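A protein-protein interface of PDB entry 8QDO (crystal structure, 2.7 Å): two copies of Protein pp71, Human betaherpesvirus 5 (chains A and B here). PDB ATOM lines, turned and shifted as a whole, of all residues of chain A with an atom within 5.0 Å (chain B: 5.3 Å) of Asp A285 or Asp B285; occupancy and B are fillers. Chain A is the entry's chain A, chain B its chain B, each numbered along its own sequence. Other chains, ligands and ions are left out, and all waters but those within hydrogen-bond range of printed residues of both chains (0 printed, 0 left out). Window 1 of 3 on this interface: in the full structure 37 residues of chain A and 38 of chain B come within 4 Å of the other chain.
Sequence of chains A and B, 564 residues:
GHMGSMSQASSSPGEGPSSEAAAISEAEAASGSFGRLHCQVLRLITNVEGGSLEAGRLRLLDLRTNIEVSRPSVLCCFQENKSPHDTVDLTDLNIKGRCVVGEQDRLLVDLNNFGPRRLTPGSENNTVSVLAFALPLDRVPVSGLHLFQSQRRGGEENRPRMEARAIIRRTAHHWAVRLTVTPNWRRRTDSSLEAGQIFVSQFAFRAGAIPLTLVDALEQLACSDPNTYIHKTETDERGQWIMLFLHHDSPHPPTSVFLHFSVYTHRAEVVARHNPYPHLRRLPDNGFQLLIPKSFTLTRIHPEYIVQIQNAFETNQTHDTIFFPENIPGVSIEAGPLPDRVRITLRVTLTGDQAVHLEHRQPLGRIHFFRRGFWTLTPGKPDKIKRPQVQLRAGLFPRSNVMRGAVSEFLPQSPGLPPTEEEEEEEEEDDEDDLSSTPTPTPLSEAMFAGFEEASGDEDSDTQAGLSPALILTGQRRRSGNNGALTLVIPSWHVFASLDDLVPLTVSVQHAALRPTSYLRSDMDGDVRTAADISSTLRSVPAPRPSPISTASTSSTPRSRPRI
NE of Arg A139 lies close to NH1 of Arg B139 (2.9 Å).
N of Val B140 is in hydrogen-bond range of O of Asp B285 (3.0 Å).
N of Val A140 lies within hydrogen-bond range of O of Asp A285.
NH2 of Arg A139 touches CG of Pro B141, 3.5 Å away.
Pro A284 touches Pro B284.
OD1 of Asp A285 touches OD1 of Asp B285 (3.8 Å).
Pro A141 touches none of the printed residues of chain B.
Asp A285 touches just one residue of chain B: Asp B285.
Printed residues of chain A within 4 Å of Arg B139: Arg A139 (2.9 Å).
Printed residues of chain A within 4 Å of Pro B141: Arg A139 (3.5 Å).
Asp B285 touches just one residue of chain A: Asp A285.
The nearest residue of chain B that does not touch Asp A285 is Pro B284 (4.9 Å).
The nearest residue of chain A that does not touch Asp B285 is Arg A139 (4.8 Å).
Hydrophobic or aromatic side chains of chain A that line the printed part of chain B: Pro A284.
Printed residues of chain B that touch a printed residue of chain A: Arg B139, Pro B141, Pro B284 and Asp B285.
Among the printed residues, no Asp or Glu carboxylate lies within 4 Å of a Lys or Arg side-chain nitrogen of the other chain.
Arg B139 touches its own counterpart, Arg A139.
Arg A139 touches Pro B141, but with the chains exchanged Pro A141 does not touch Arg B139 (5.0 Å).
Pro B284 touches its own counterpart, Pro A284.
Asp A285 touches its own counterpart, Asp B285.
Of the 4 pairs that touch across the chains among the printed residues, 3 have their exchanged pair printed and touching as well.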
ATOM      1  N   ASP A 138     -31.102 -13.916 -26.546  1.00  0.00           N
ATOM      2  CA  ASP A 138     -31.370 -12.556 -26.106  1.00  0.00           C
ATOM      3  C   ASP A 138     -30.387 -12.153 -25.011  1.00  0.00           C
ATOM      4  O   ASP A 138     -29.722 -12.989 -24.395  1.00  0.00           O
ATOM      5  CB  ASP A 138     -32.801 -12.420 -25.587  1.00  0.00           C
ATOM      6  CG  ASP A 138     -33.835 -12.703 -26.660  1.00  0.00           C
ATOM      7  OD1 ASP A 138     -33.691 -12.161 -27.779  1.00  0.00           O
ATOM      8  OD2 ASP A 138     -34.803 -13.445 -26.376  1.00  0.00           O
ATOM      9  N   ARG A 139     -30.296 -10.848 -24.773  1.00  0.00           N
ATOM     10  CA  ARG A 139     -29.369 -10.319 -23.776  1.00  0.00           C
ATOM     11  C   ARG A 139     -29.971 -10.511 -22.386  1.00  0.00           C
ATOM     12  O   ARG A 139     -31.016  -9.936 -22.066  1.00  0.00           O
ATOM     13  CB  ARG A 139     -29.051  -8.862 -24.091  1.00  0.00           C
ATOM     14  CG  ARG A 139     -27.945  -8.222 -23.263  1.00  0.00           C
ATOM     15  CD  ARG A 139     -27.551  -6.878 -23.886  1.00  0.00           C
ATOM     16  NE  ARG A 139     -28.567  -5.835 -23.784  1.00  0.00           N
ATOM     17  CZ  ARG A 139     -28.504  -4.671 -24.423  1.00  0.00           C
ATOM     18  NH1 ARG A 139     -27.497  -4.380 -25.236  1.00  0.00           N
ATOM     19  NH2 ARG A 139     -29.472  -3.775 -24.239  1.00  0.00           N
ATOM     20  N   VAL A 140     -29.338 -11.349 -21.576  1.00  0.00           N
ATOM     21  CA  VAL A 140     -29.792 -11.624 -20.220  1.00  0.00           C
ATOM     22  C   VAL A 140     -28.662 -11.304 -19.251  1.00  0.00           C
ATOM     23  O   VAL A 140     -27.697 -12.059 -19.136  1.00  0.00           O
ATOM     24  CB  VAL A 140     -30.256 -13.081 -20.063  1.00  0.00           C
ATOM     25  CG1 VAL A 140     -30.683 -13.325 -18.628  1.00  0.00           C
ATOM     26  CG2 VAL A 140     -31.390 -13.362 -21.010  1.00  0.00           C
ATOM     27  N   PRO A 141     -28.743 -10.182 -18.541  1.00  0.00           N
ATOM     28  CA  PRO A 141     -27.703  -9.867 -17.555  1.00  0.00           C
ATOM     29  C   PRO A 141     -27.801 -10.771 -16.334  1.00  0.00           C
ATOM     30  O   PRO A 141     -28.888 -11.169 -15.911  1.00  0.00           O
ATOM     31  CB  PRO A 141     -27.993  -8.405 -17.193  1.00  0.00           C
ATOM     32  CG  PRO A 141     -29.457  -8.244 -17.471  1.00  0.00           C
ATOM     33  CD  PRO A 141     -29.741  -9.103 -18.666  1.00  0.00           C
ATOM     34  N   LEU A 283     -19.861 -15.070 -21.023  1.00  0.00           N
ATOM     35  CA  LEU A 283     -19.959 -14.909 -22.465  1.00  0.00           C
ATOM     36  C   LEU A 283     -20.674 -13.601 -22.807  1.00  0.00           C
ATOM     37  O   LEU A 283     -21.466 -13.090 -22.008  1.00  0.00           O
ATOM     38  CB  LEU A 283     -20.717 -16.082 -23.092  1.00  0.00           C
ATOM     39  CG  LEU A 283     -20.086 -17.470 -23.035  1.00  0.00           C
ATOM     40  CD1 LEU A 283     -21.074 -18.523 -23.508  1.00  0.00           C
ATOM     41  CD2 LEU A 283     -18.822 -17.533 -23.873  1.00  0.00           C
ATOM     42  N   PRO A 284     -20.414 -13.026 -23.975  1.00  0.00           N
ATOM     43  CA  PRO A 284     -21.071 -11.760 -24.326  1.00  0.00           C
ATOM     44  C   PRO A 284     -22.581 -11.931 -24.460  1.00  0.00           C
ATOM     45  O   PRO A 284     -23.061 -12.816 -25.174  1.00  0.00           O
ATOM     46  CB  PRO A 284     -20.424 -11.388 -25.667  1.00  0.00           C
ATOM     47  CG  PRO A 284     -19.996 -12.716 -26.248  1.00  0.00           C
ATOM     48  CD  PRO A 284     -19.523 -13.500 -25.050  1.00  0.00           C
ATOM     49  N   ASP A 285     -23.326 -11.044 -23.787  1.00  0.00           N
ATOM     50  CA  ASP A 285     -24.782 -10.948 -23.885  1.00  0.00           C
ATOM     51  C   ASP A 285     -25.544 -12.029 -23.134  1.00  0.00           C
ATOM     52  O   ASP A 285     -26.512 -11.721 -22.429  1.00  0.00           O
ATOM     53  CB  ASP A 285     -25.236 -10.963 -25.344  1.00  0.00           C
ATOM     54  CG  ASP A 285     -24.867  -9.692 -26.081  1.00  0.00           C
ATOM     55  OD1 ASP A 285     -25.077  -8.598 -25.512  1.00  0.00           O
ATOM     56  OD2 ASP A 285     -24.375  -9.790 -27.234  1.00  0.00           O
ATOM     57  N   ASN A 286     -25.186 -13.295 -23.334  1.00  0.00           N
ATOM     58  CA  ASN A 286     -25.972 -14.377 -22.759  1.00  0.00           C
ATOM     59  C   ASN A 286     -25.094 -15.573 -22.417  1.00  0.00           C
ATOM     60  O   ASN A 286     -24.403 -16.109 -23.288  1.00  0.00           O
ATOM     61  CB  ASN A 286     -27.088 -14.781 -23.731  1.00  0.00           C
ATOM     62  CG  ASN A 286     -27.996 -15.869 -23.180  1.00  0.00           C
ATOM     63  OD1 ASN A 286     -27.534 -16.909 -22.700  1.00  0.00           O
ATOM     64  ND2 ASN A 286     -29.303 -15.638 -23.262  1.00  0.00           N
ATOM     65  N   GLY A 287     -25.159 -16.013 -21.155  1.00  0.00           N
ATOM     66  CA  GLY A 287     -24.622 -17.301 -20.761  1.00  0.00           C
ATOM     67  C   GLY A 287     -23.179 -17.318 -20.300  1.00  0.00           C
ATOM     68  O   GLY A 287     -22.485 -16.298 -20.188  1.00  0.00           O
ATOM     69  N   ASP B 138     -18.902   0.573 -20.819  1.00  0.00           N
ATOM     70  CA  ASP B 138     -20.246   0.224 -20.385  1.00  0.00           C
ATOM     71  C   ASP B 138     -21.098  -0.215 -21.574  1.00  0.00           C
ATOM     72  O   ASP B 138     -20.733  -0.025 -22.741  1.00  0.00           O
ATOM     73  CB  ASP B 138     -20.901   1.404 -19.675  1.00  0.00           C
ATOM     74  CG  ASP B 138     -20.168   1.795 -18.414  1.00  0.00           C
ATOM     75  OD1 ASP B 138     -19.868   0.894 -17.600  1.00  0.00           O
ATOM     76  OD2 ASP B 138     -19.901   3.001 -18.238  1.00  0.00           O
ATOM     77  N   ARG B 139     -22.244  -0.825 -21.269  1.00  0.00           N
ATOM     78  CA  ARG B 139     -23.134  -1.339 -22.306  1.00  0.00           C
ATOM     79  C   ARG B 139     -23.920  -0.187 -22.927  1.00  0.00           C
ATOM     80  O   ARG B 139     -24.653   0.516 -22.223  1.00  0.00           O
ATOM     81  CB  ARG B 139     -24.115  -2.366 -21.756  1.00  0.00           C
ATOM     82  CG  ARG B 139     -24.829  -3.099 -22.887  1.00  0.00           C
ATOM     83  CD  ARG B 139     -25.933  -4.016 -22.409  1.00  0.00           C
ATOM     84  NE  ARG B 139     -27.067  -3.205 -21.974  1.00  0.00           N
ATOM     85  CZ  ARG B 139     -28.148  -3.668 -21.360  1.00  0.00           C
ATOM     86  NH1 ARG B 139     -28.286  -4.954 -21.072  1.00  0.00           N
ATOM     87  NH2 ARG B 139     -29.115  -2.815 -21.029  1.00  0.00           N
ATOM     88  N   VAL B 140     -23.737   0.047 -24.219  1.00  0.00           N
ATOM     89  CA  VAL B 140     -24.460   1.089 -24.934  1.00  0.00           C
ATOM     90  C   VAL B 140     -25.165   0.467 -26.137  1.00  0.00           C
ATOM     91  O   VAL B 140     -24.543   0.194 -27.165  1.00  0.00           O
ATOM     92  CB  VAL B 140     -23.521   2.226 -25.363  1.00  0.00           C
ATOM     93  CG1 VAL B 140     -24.303   3.287 -26.120  1.00  0.00           C
ATOM     94  CG2 VAL B 140     -22.825   2.803 -24.134  1.00  0.00           C
ATOM     95  N   PRO B 141     -26.476   0.266 -26.057  1.00  0.00           N
ATOM     96  CA  PRO B 141     -27.205  -0.309 -27.192  1.00  0.00           C
ATOM     97  C   PRO B 141     -27.274   0.662 -28.358  1.00  0.00           C
ATOM     98  O   PRO B 141     -27.315   1.881 -28.176  1.00  0.00           O
ATOM     99  CB  PRO B 141     -28.602  -0.582 -26.617  1.00  0.00           C
ATOM    100  CG  PRO B 141     -28.419  -0.592 -25.136  1.00  0.00           C
ATOM    101  CD  PRO B 141     -27.311   0.355 -24.846  1.00  0.00           C
ATOM    102  N   LEU B 283     -19.620  -4.859 -32.195  1.00  0.00           N
ATOM    103  CA  LEU B 283     -18.859  -5.476 -31.121  1.00  0.00           C
ATOM    104  C   LEU B 283     -19.772  -5.764 -29.930  1.00  0.00           C
ATOM    105  O   LEU B 283     -20.794  -5.093 -29.747  1.00  0.00           O
ATOM    106  CB  LEU B 283     -17.701  -4.585 -30.659  1.00  0.00           C
ATOM    107  CG  LEU B 283     -16.565  -4.341 -31.653  1.00  0.00           C
ATOM    108  CD1 LEU B 283     -15.618  -3.280 -31.124  1.00  0.00           C
ATOM    109  CD2 LEU B 283     -15.811  -5.628 -31.925  1.00  0.00           C
ATOM    110  N   PRO B 284     -19.437  -6.753 -29.103  1.00  0.00           N
ATOM    111  CA  PRO B 284     -20.306  -7.080 -27.966  1.00  0.00           C
ATOM    112  C   PRO B 284     -20.377  -5.929 -26.971  1.00  0.00           C
ATOM    113  O   PRO B 284     -19.353  -5.373 -26.563  1.00  0.00           O
ATOM    114  CB  PRO B 284     -19.632  -8.312 -27.355  1.00  0.00           C
ATOM    115  CG  PRO B 284     -18.185  -8.169 -27.747  1.00  0.00           C
ATOM    116  CD  PRO B 284     -18.239  -7.608 -29.142  1.00  0.00           C
ATOM    117  N   ASP B 285     -21.608  -5.570 -26.591  1.00  0.00           N
ATOM    118  CA  ASP B 285     -21.877  -4.595 -25.534  1.00  0.00           C
ATOM    119  C   ASP B 285     -21.624  -3.147 -25.930  1.00  0.00           C
ATOM    120  O   ASP B 285     -22.470  -2.284 -25.669  1.00  0.00           O
ATOM    121  CB  ASP B 285     -21.067  -4.929 -24.285  1.00  0.00           C
ATOM    122  CG  ASP B 285     -21.548  -6.199 -23.616  1.00  0.00           C
ATOM    123  OD1 ASP B 285     -22.785  -6.375 -23.474  1.00  0.00           O
ATOM    124  OD2 ASP B 285     -20.686  -7.024 -23.246  1.00  0.00           O
ATOM    125  N   ASN B 286     -20.457  -2.842 -26.501  1.00  0.00           N
ATOM    126  CA  ASN B 286     -20.128  -1.446 -26.773  1.00  0.00           C
ATOM    127  C   ASN B 286     -19.278  -1.320 -28.029  1.00  0.00           C
ATOM    128  O   ASN B 286     -18.195  -1.909 -28.114  1.00  0.00           O
ATOM    129  CB  ASN B 286     -19.395  -0.823 -25.576  1.00  0.00           C
ATOM    130  CG  ASN B 286     -19.079   0.652 -25.776  1.00  0.00           C
ATOM    131  OD1 ASN B 286     -18.525   1.053 -26.805  1.00  0.00           O
ATOM    132  ND2 ASN B 286     -19.413   1.462 -24.782  1.00  0.00           N
ATOM    133  N   GLY B 287     -19.754  -0.510 -28.982  1.00  0.00           N
ATOM    134  CA  GLY B 287     -18.931  -0.060 -30.085  1.00  0.00           C
ATOM    135  C   GLY B 287     -18.927  -0.938 -31.320  1.00  0.00           C
ATOM    136  O   GLY B 287     -19.592  -1.975 -31.423  1.00  0.00           O
